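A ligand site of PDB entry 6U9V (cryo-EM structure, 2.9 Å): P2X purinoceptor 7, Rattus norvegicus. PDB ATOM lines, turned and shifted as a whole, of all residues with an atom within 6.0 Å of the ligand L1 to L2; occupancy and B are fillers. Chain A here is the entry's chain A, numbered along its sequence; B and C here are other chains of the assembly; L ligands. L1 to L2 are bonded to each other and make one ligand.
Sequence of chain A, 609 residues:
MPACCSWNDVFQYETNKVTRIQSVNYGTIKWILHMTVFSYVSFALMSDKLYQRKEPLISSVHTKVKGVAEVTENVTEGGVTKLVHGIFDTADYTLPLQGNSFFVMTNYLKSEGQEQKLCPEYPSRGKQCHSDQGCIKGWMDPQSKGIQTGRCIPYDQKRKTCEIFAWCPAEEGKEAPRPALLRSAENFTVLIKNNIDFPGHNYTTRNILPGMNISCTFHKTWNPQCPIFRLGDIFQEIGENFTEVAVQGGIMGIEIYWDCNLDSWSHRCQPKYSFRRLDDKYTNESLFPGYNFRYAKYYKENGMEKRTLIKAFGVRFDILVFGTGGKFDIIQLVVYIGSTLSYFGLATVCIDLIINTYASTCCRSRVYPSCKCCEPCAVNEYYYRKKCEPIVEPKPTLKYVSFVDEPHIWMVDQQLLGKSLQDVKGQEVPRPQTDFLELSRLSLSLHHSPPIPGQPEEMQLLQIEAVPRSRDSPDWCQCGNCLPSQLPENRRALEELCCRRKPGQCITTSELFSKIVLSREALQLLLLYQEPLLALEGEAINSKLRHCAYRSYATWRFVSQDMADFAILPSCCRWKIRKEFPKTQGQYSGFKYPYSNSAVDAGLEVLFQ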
ATOM      1  N   ARG A  20     -19.778 -26.899  -3.503  1.00  0.00           N
ATOM      2  CA  ARG A  20     -19.956 -25.495  -3.150  1.00  0.00           C
ATOM      3  C   ARG A  20     -18.923 -25.119  -2.093  1.00  0.00           C
ATOM      4  O   ARG A  20     -19.013 -25.559  -0.941  1.00  0.00           O
ATOM      5  CB  ARG A  20     -21.379 -25.255  -2.648  1.00  0.00           C
ATOM      6  CG  ARG A  20     -21.800 -23.796  -2.612  1.00  0.00           C
ATOM      7  CD  ARG A  20     -23.151 -23.644  -1.947  1.00  0.00           C
ATOM      8  NE  ARG A  20     -24.040 -22.738  -2.678  1.00  0.00           N
ATOM      9  CZ  ARG A  20     -24.734 -23.066  -3.765  1.00  0.00           C
ATOM     10  NH1 ARG A  20     -25.508 -22.152  -4.339  1.00  0.00           N
ATOM     11  NH2 ARG A  20     -24.667 -24.288  -4.288  1.00  0.00           N
ATOM     12  N   LYS A  30     -14.525 -14.028  -7.702  1.00  0.00           N
ATOM     13  CA  LYS A  30     -15.530 -14.410  -8.681  1.00  0.00           C
ATOM     14  C   LYS A  30     -16.457 -13.239  -9.001  1.00  0.00           C
ATOM     15  O   LYS A  30     -16.656 -12.889 -10.178  1.00  0.00           O
ATOM     16  CB  LYS A  30     -16.331 -15.601  -8.149  1.00  0.00           C
ATOM     17  CG  LYS A  30     -17.340 -16.221  -9.110  1.00  0.00           C
ATOM     18  CD  LYS A  30     -18.449 -16.906  -8.342  1.00  0.00           C
ATOM     19  CE  LYS A  30     -19.411 -17.638  -9.259  1.00  0.00           C
ATOM     20  NZ  LYS A  30     -20.524 -18.287  -8.514  1.00  0.00           N
ATOM     21  N   TRP A  31     -17.013 -12.608  -7.969  1.00  0.00           N
ATOM     22  CA  TRP A  31     -17.993 -11.568  -8.191  1.00  0.00           C
ATOM     23  C   TRP A  31     -17.365 -10.322  -8.805  1.00  0.00           C
ATOM     24  O   TRP A  31     -17.953  -9.705  -9.699  1.00  0.00           O
ATOM     25  CB  TRP A  31     -18.707 -11.215  -6.881  1.00  0.00           C
ATOM     26  CG  TRP A  31     -19.748 -12.222  -6.500  1.00  0.00           C
ATOM     27  CD1 TRP A  31     -19.764 -12.993  -5.366  1.00  0.00           C
ATOM     28  CD2 TRP A  31     -20.931 -12.569  -7.231  1.00  0.00           C
ATOM     29  NE1 TRP A  31     -20.883 -13.796  -5.356  1.00  0.00           N
ATOM     30  CE2 TRP A  31     -21.605 -13.561  -6.494  1.00  0.00           C
ATOM     31  CE3 TRP A  31     -21.468 -12.146  -8.455  1.00  0.00           C
ATOM     32  CZ2 TRP A  31     -22.808 -14.119  -6.929  1.00  0.00           C
ATOM     33  CZ3 TRP A  31     -22.662 -12.709  -8.882  1.00  0.00           C
ATOM     34  CH2 TRP A  31     -23.312 -13.689  -8.118  1.00  0.00           C
ATOM     35  N   HIS A  34     -16.666 -11.103 -12.501  1.00  0.00           N
ATOM     36  CA  HIS A  34     -17.917 -11.060 -13.256  1.00  0.00           C
ATOM     37  C   HIS A  34     -18.393  -9.626 -13.454  1.00  0.00           C
ATOM     38  O   HIS A  34     -18.819  -9.256 -14.550  1.00  0.00           O
ATOM     39  CB  HIS A  34     -18.987 -11.882 -12.540  1.00  0.00           C
ATOM     40  CG  HIS A  34     -18.761 -13.369 -12.612  1.00  0.00           C
ATOM     41  ND1 HIS A  34     -19.630 -14.270 -12.046  1.00  0.00           N
ATOM     42  CD2 HIS A  34     -17.773 -14.091 -13.184  1.00  0.00           C
ATOM     43  CE1 HIS A  34     -19.183 -15.498 -12.262  1.00  0.00           C
ATOM     44  NE2 HIS A  34     -18.055 -15.407 -12.952  1.00  0.00           N
ATOM     45  N   PHE A 344     -17.518 -14.825 -19.240  1.00  0.00           N
ATOM     46  CA  PHE A 344     -17.965 -15.000 -17.865  1.00  0.00           C
ATOM     47  C   PHE A 344     -17.333 -16.214 -17.191  1.00  0.00           C
ATOM     48  O   PHE A 344     -17.341 -16.280 -15.956  1.00  0.00           O
ATOM     49  CB  PHE A 344     -19.493 -15.135 -17.824  1.00  0.00           C
ATOM     50  CG  PHE A 344     -20.213 -13.857 -18.154  1.00  0.00           C
ATOM     51  CD1 PHE A 344     -20.393 -12.876 -17.194  1.00  0.00           C
ATOM     52  CD2 PHE A 344     -20.697 -13.634 -19.435  1.00  0.00           C
ATOM     53  CE1 PHE A 344     -21.054 -11.707 -17.493  1.00  0.00           C
ATOM     54  CE2 PHE A 344     -21.358 -12.458 -19.741  1.00  0.00           C
ATOM     55  CZ  PHE A 344     -21.535 -11.498 -18.773  1.00  0.00           C
ATOM     56  N   ASP B   9     -24.260 -16.966   1.501  1.00  0.00           N
ATOM     57  CA  ASP B   9     -24.613 -17.469   0.181  1.00  0.00           C
ATOM     58  C   ASP B   9     -23.951 -16.678  -0.934  1.00  0.00           C
ATOM     59  O   ASP B   9     -23.808 -17.202  -2.049  1.00  0.00           O
ATOM     60  CB  ASP B   9     -26.137 -17.436   0.008  1.00  0.00           C
ATOM     61  N   VAL B  10     -23.557 -15.433  -0.679  1.00  0.00           N
ATOM     62  CA  VAL B  10     -22.925 -14.617  -1.713  1.00  0.00           C
ATOM     63  C   VAL B  10     -21.493 -15.079  -1.956  1.00  0.00           C
ATOM     64  O   VAL B  10     -20.993 -15.023  -3.086  1.00  0.00           O
ATOM     65  CB  VAL B  10     -22.972 -13.127  -1.321  1.00  0.00           C
ATOM     66  CG1 VAL B  10     -22.177 -12.291  -2.310  1.00  0.00           C
ATOM     67  CG2 VAL B  10     -24.421 -12.645  -1.238  1.00  0.00           C
ATOM     68  N   PHE B  11     -20.809 -15.549  -0.906  1.00  0.00           N
ATOM     69  CA  PHE B  11     -19.410 -15.977  -1.005  1.00  0.00           C
ATOM     70  C   PHE B  11     -19.264 -17.446  -1.393  1.00  0.00           C
ATOM     71  O   PHE B  11     -18.221 -18.045  -1.119  1.00  0.00           O
ATOM     72  CB  PHE B  11     -18.695 -15.710   0.316  1.00  0.00           C
ATOM     73  CG  PHE B  11     -18.797 -14.286   0.798  1.00  0.00           C
ATOM     74  CD1 PHE B  11     -18.713 -13.225  -0.083  1.00  0.00           C
ATOM     75  CD2 PHE B  11     -18.982 -14.010   2.147  1.00  0.00           C
ATOM     76  CE1 PHE B  11     -18.806 -11.909   0.364  1.00  0.00           C
ATOM     77  CE2 PHE B  11     -19.072 -12.715   2.602  1.00  0.00           C
ATOM     78  CZ  PHE B  11     -18.986 -11.661   1.714  1.00  0.00           C
ATOM     79  N   GLN B  12     -20.280 -18.037  -2.017  1.00  0.00           N
ATOM     80  CA  GLN B  12     -20.226 -19.418  -2.457  1.00  0.00           C
ATOM     81  C   GLN B  12     -19.694 -19.488  -3.891  1.00  0.00           C
ATOM     82  O   GLN B  12     -20.116 -18.705  -4.753  1.00  0.00           O
ATOM     83  CB  GLN B  12     -21.605 -20.078  -2.386  1.00  0.00           C
ATOM     84  CG  GLN B  12     -22.238 -20.068  -1.007  1.00  0.00           C
ATOM     85  CD  GLN B  12     -21.481 -20.899   0.010  1.00  0.00           C
ATOM     86  OE1 GLN B  12     -20.547 -21.625  -0.328  1.00  0.00           O
ATOM     87  NE2 GLN B  12     -21.883 -20.800   1.274  1.00  0.00           N
ATOM     88  N   TYR B  13     -18.778 -20.417  -4.119  1.00  0.00           N
ATOM     89  CA  TYR B  13     -18.228 -20.675  -5.443  1.00  0.00           C
ATOM     90  C   TYR B  13     -18.257 -22.169  -5.698  1.00  0.00           C
ATOM     91  O   TYR B  13     -17.844 -22.954  -4.838  1.00  0.00           O
ATOM     92  CB  TYR B  13     -16.800 -20.137  -5.578  1.00  0.00           C
ATOM     93  CG  TYR B  13     -16.102 -20.607  -6.834  1.00  0.00           C
ATOM     94  CD1 TYR B  13     -16.429 -20.084  -8.076  1.00  0.00           C
ATOM     95  CD2 TYR B  13     -15.117 -21.579  -6.768  1.00  0.00           C
ATOM     96  CE1 TYR B  13     -15.792 -20.513  -9.221  1.00  0.00           C
ATOM     97  CE2 TYR B  13     -14.471 -22.013  -7.904  1.00  0.00           C
ATOM     98  CZ  TYR B  13     -14.816 -21.471  -9.128  1.00  0.00           C
ATOM     99  OH  TYR B  13     -14.168 -21.912 -10.256  1.00  0.00           O
ATOM    100  N   GLU B  14     -18.732 -22.570  -6.875  1.00  0.00           N
ATOM    101  CA  GLU B  14     -18.928 -23.973  -7.233  1.00  0.00           C
ATOM    102  C   GLU B  14     -17.899 -24.368  -8.283  1.00  0.00           C
ATOM    103  O   GLU B  14     -17.921 -23.865  -9.412  1.00  0.00           O
ATOM    104  CB  GLU B  14     -20.352 -24.197  -7.756  1.00  0.00           C
ATOM    105  CG  GLU B  14     -21.433 -23.857  -6.744  1.00  0.00           C
ATOM    106  CD  GLU B  14     -22.827 -24.111  -7.284  1.00  0.00           C
ATOM    107  OE1 GLU B  14     -22.948 -24.518  -8.460  1.00  0.00           O
ATOM    108  OE2 GLU B  14     -23.810 -23.910  -6.536  1.00  0.00           O
ATOM    109  N   VAL C 349     -28.440 -23.897 -18.017  1.00  0.00           N
ATOM    110  CA  VAL C 349     -28.519 -22.822 -17.037  1.00  0.00           C
ATOM    111  C   VAL C 349     -29.906 -22.766 -16.408  1.00  0.00           C
ATOM    112  O   VAL C 349     -30.050 -22.666 -15.190  1.00  0.00           O
ATOM    113  CB  VAL C 349     -28.134 -21.475 -17.688  1.00  0.00           C
ATOM    114  CG1 VAL C 349     -28.492 -20.302 -16.773  1.00  0.00           C
ATOM    115  CG2 VAL C 349     -26.647 -21.444 -18.010  1.00  0.00           C
ATOM    116  N   ASP C 352     -30.484 -25.859 -14.118  1.00  0.00           N
ATOM    117  CA  ASP C 352     -29.736 -25.718 -12.879  1.00  0.00           C
ATOM    118  C   ASP C 352     -30.367 -24.673 -11.972  1.00  0.00           C
ATOM    119  O   ASP C 352     -30.400 -24.853 -10.750  1.00  0.00           O
ATOM    120  CB  ASP C 352     -28.282 -25.360 -13.175  1.00  0.00           C
ATOM    121  CG  ASP C 352     -27.554 -26.467 -13.921  1.00  0.00           C
ATOM    122  OD1 ASP C 352     -28.175 -27.500 -14.202  1.00  0.00           O
ATOM    123  OD2 ASP C 352     -26.353 -26.284 -14.216  1.00  0.00           O
ATOM    124  N   LEU C 353     -30.877 -23.582 -12.546  1.00  0.00           N
ATOM    125  CA  LEU C 353     -31.589 -22.587 -11.755  1.00  0.00           C
ATOM    126  C   LEU C 353     -32.836 -23.188 -11.127  1.00  0.00           C
ATOM    127  O   LEU C 353     -33.140 -22.935  -9.952  1.00  0.00           O
ATOM    128  CB  LEU C 353     -31.940 -21.386 -12.644  1.00  0.00           C
ATOM    129  CG  LEU C 353     -32.774 -20.261 -12.019  1.00  0.00           C
ATOM    130  CD1 LEU C 353     -32.115 -19.726 -10.756  1.00  0.00           C
ATOM    131  CD2 LEU C 353     -32.970 -19.140 -13.030  1.00  0.00           C
ATOM    132  N   ASN C 356     -31.718 -25.493  -8.245  1.00  0.00           N
ATOM    133  CA  ASN C 356     -31.239 -24.752  -7.086  1.00  0.00           C
ATOM    134  C   ASN C 356     -32.354 -23.967  -6.407  1.00  0.00           C
ATOM    135  O   ASN C 356     -32.267 -23.725  -5.196  1.00  0.00           O
ATOM    136  CB  ASN C 356     -30.118 -23.795  -7.504  1.00  0.00           C
ATOM    137  CG  ASN C 356     -28.902 -24.528  -8.062  1.00  0.00           C
ATOM    138  OD1 ASN C 356     -28.650 -25.679  -7.709  1.00  0.00           O
ATOM    139  ND2 ASN C 356     -28.165 -23.866  -8.927  1.00  0.00           N
HETATM  140  C1  LIG L   1     -23.764 -17.604 -12.988  1.00  0.00           C
HETATM  141  C2  LIG L   1     -23.251 -16.997 -11.695  1.00  0.00           C
HETATM  142  C3  LIG L   1     -23.746 -17.758 -10.512  1.00  0.00           C
HETATM  143  C4  LIG L   1     -25.224 -18.062 -10.651  1.00  0.00           C
HETATM  144  C5  LIG L   1     -25.470 -19.014 -11.812  1.00  0.00           C
HETATM  145  C6  LIG L   1     -26.743 -18.627 -12.511  1.00  0.00           C
HETATM  146  O1  LIG L   1     -22.743 -17.686 -13.858  1.00  0.00           O
HETATM  147  O2  LIG L   1     -21.818 -17.032 -11.704  1.00  0.00           O
HETATM  148  O3  LIG L   1     -23.531 -16.977  -9.323  1.00  0.00           O
HETATM  149  O4  LIG L   1     -25.825 -18.562  -9.421  1.00  0.00           O
HETATM  150  O5  LIG L   1     -24.357 -18.986 -12.800  1.00  0.00           O
HETATM  151  O6  LIG L   1     -27.034 -19.583 -13.478  1.00  0.00           O
HETATM  152  C1  LG2 L   2     -25.115 -19.565  -8.738  1.00  0.00           C
HETATM  153  C2  LG2 L   2     -26.106 -20.435  -8.001  1.00  0.00           C
HETATM  154  C3  LG2 L   2     -26.779 -19.704  -6.896  1.00  0.00           C
HETATM  155  C4  LG2 L   2     -25.790 -19.066  -5.961  1.00  0.00           C
HETATM  156  C5  LG2 L   2     -24.774 -18.205  -6.708  1.00  0.00           C
HETATM  157  C6  LG2 L   2     -23.734 -17.751  -5.728  1.00  0.00           C
HETATM  158  O1  LG2 L   2     -27.110 -20.902  -8.938  1.00  0.00           O
HETATM  159  O2  LG2 L   2     -27.594 -20.638  -6.141  1.00  0.00           O
HETATM  160  O3  LG2 L   2     -26.504 -18.240  -5.028  1.00  0.00           O
HETATM  161  O4  LG2 L   2     -24.123 -18.934  -7.809  1.00  0.00           O
HETATM  162  O5  LG2 L   2     -24.353 -17.545  -4.424  1.00  0.00           O
HETATM  163  C1  LG3 L   3     -24.833  -8.209 -21.460  1.00  0.00           C
HETATM  164  C2  LG3 L   3     -24.757 -11.715 -19.865  1.00  0.00           C
HETATM  165  C3  LG3 L   3     -25.257 -14.015 -18.899  1.00  0.00           C
HETATM  166  C4  LG3 L   3     -25.416 -15.711 -17.001  1.00  0.00           C
HETATM  167  C5  LG3 L   3     -23.058 -17.790 -19.079  1.00  0.00           C
HETATM  168  C6  LG3 L   3     -23.310 -19.038 -19.927  1.00  0.00           C
HETATM  169  C7  LG3 L   3     -24.531  -6.947 -21.228  1.00  0.00           C
HETATM  170  C8  LG3 L   3     -24.809  -9.224 -20.314  1.00  0.00           C
HETATM  171  C9  LG3 L   3     -25.296 -10.596 -20.761  1.00  0.00           C
HETATM  172  C10 LG3 L   3     -25.844 -12.731 -19.506  1.00  0.00           C
HETATM  173  C11 LG3 L   3     -26.059 -14.514 -17.706  1.00  0.00           C
HETATM  174  C12 LG3 L   3     -24.183 -16.249 -17.706  1.00  0.00           C
HETATM  175  C13 LG3 L   3     -22.504 -20.252 -19.465  1.00  0.00           C
HETATM  176  C14 LG3 L   3     -18.807 -21.329 -16.600  1.00  0.00           C
HETATM  177  C15 LG3 L   3     -18.540 -22.779 -16.204  1.00  0.00           C
HETATM  178  C16 LG3 L   3     -17.908 -23.584 -17.338  1.00  0.00           C
HETATM  179  C17 LG3 L   3     -25.401 -19.121 -20.997  1.00  0.00           C
HETATM  180  C18 LG3 L   3     -26.926 -19.242 -20.984  1.00  0.00           C
HETATM  181  C19 LG3 L   3     -27.557 -18.681 -22.253  1.00  0.00           C
HETATM  182  C20 LG3 L   3     -27.355 -17.169 -22.390  1.00  0.00           C
HETATM  183  C21 LG3 L   3     -28.388 -16.377 -21.596  1.00  0.00           C
HETATM  184  C22 LG3 L   3     -28.626 -14.992 -22.181  1.00  0.00           C
HETATM  185  C23 LG3 L   3     -30.096 -14.587 -22.118  1.00  0.00           C
HETATM  186  C24 LG3 L   3     -30.625 -14.101 -23.463  1.00  0.00           C
HETATM  187  C25 LG3 L   3     -32.148 -14.042 -23.499  1.00  0.00           C
HETATM  188  N1  LG3 L   3     -19.781 -23.407 -15.798  1.00  0.00           N
HETATM  189  O1  LG3 L   3     -23.144 -15.670 -17.639  1.00  0.00           O
HETATM  190  O2  LG3 L   3     -24.258 -17.436 -18.456  1.00  0.00           O
HETATM  191  O3  LG3 L   3     -22.286 -20.137 -18.087  1.00  0.00           O
HETATM  192  O4  LG3 L   3     -20.772 -19.146 -16.246  1.00  0.00           O
HETATM  193  O5  LG3 L   3     -20.022 -19.003 -18.595  1.00  0.00           O
HETATM  194  O6  LG3 L   3     -19.943 -21.292 -17.406  1.00  0.00           O
HETATM  195  O7  LG3 L   3     -18.489 -24.600 -17.799  1.00  0.00           O
HETATM  196  O8  LG3 L   3     -16.794 -23.223 -17.820  1.00  0.00           O
HETATM  197  O9  LG3 L   3     -24.674 -19.362 -19.822  1.00  0.00           O
HETATM  198  O10 LG3 L   3     -24.832 -18.823 -21.989  1.00  0.00           O
HETATM  199  P1  LG3 L   3     -20.735 -19.865 -17.576  1.00  0.00           P
HETATM  200  C1  LG4 L   4     -32.519 -21.528  -1.945  1.00  0.00           C
HETATM  201  O1  LG4 L   4     -31.332 -21.772  -2.181  1.00  0.00           O
HETATM  202  C2  LG4 L   4     -33.304 -20.461  -2.634  1.00  0.00           C
HETATM  203  C3  LG4 L   4     -32.954 -20.331  -4.107  1.00  0.00           C
HETATM  204  C4  LG4 L   4     -31.978 -19.212  -4.377  1.00  0.00           C
HETATM  205  C5  LG4 L   4     -31.503 -19.257  -5.815  1.00  0.00           C
HETATM  206  C6  LG4 L   4     -30.986 -17.907  -6.283  1.00  0.00           C
HETATM  207  C7  LG4 L   4     -30.545 -17.981  -7.734  1.00  0.00           C
HETATM  208  C8  LG4 L   4     -30.263 -16.610  -8.303  1.00  0.00           C
HETATM  209  C9  LG4 L   4     -29.886 -16.705  -9.773  1.00  0.00           C
HETATM  210  C10 LG4 L   4     -29.826 -15.340 -10.426  1.00  0.00           C
HETATM  211  C11 LG4 L   4     -29.494 -15.466 -11.898  1.00  0.00           C
HETATM  212  C12 LG4 L   4     -29.490 -14.113 -12.576  1.00  0.00           C
HETATM  213  C13 LG4 L   4     -29.033 -14.220 -14.017  1.00  0.00           C
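The side-chain amide nitrogen of Asn 356 of chain C is in hydrogen-bond range of an oxygen (O1) of LG2 L2, at 3.1 Å. An oxygen (O3) of LIG L1 is in hydrogen-bond range of the side-chain amino group (NZ) of Lys 30, at 3.4 Å. An oxygen (O2) of LG2 L2 is in hydrogen-bond range of the guanidinium group (NH1) of Arg 20 (3.1 Å). The backbone carbonyl oxygen of Asp 9 of chain B is in hydrogen-bond range of an oxygen (O5) of LG2 L2.
An oxygen (O4) of LG3 L3 sits at hydrogen-bond distance from an oxygen (O1) of LIG L1.
NE1 of Trp 31 lies within hydrogen-bond range of O of Val 10 of chain B. ND2 of Asn 356 of chain C is in hydrogen-bond range of O of Asp 352 of chain C, 3.0 Å away. NH2 of Arg 20 is in salt-bridge range of OE2 of Glu 14 of chain B (2.4 Å). O of Phe 344 is in hydrogen-bond range of NE2 of His 34, 3.2 Å away.
CH2 of Trp 31 touches O3 of LIG L1, at 3.5 Å. His 34 touches the ligand L1 to L2. Gln 12 of chain B touches the ligand L1 to L2. CG1 of Val 349 of chain C touches O6 of LIG L1 (3.7 Å). Hydrophobic or aromatic side chains that line the ligand L1 to L2: Trp 31, His 34 and Val 349 of chain C. Eight residues have an atom within 4 Å of the ligand L1 to L2: Arg 20, Lys 30, Trp 31, His 34, Asp 9 of chain B, Gln 12 of chain B, Val 349 of chain C and Asn 356 of chain C. The nearest printed residue that does not touch the ligand L1 to L2 is Val 10 of chain B (4.2 Å).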
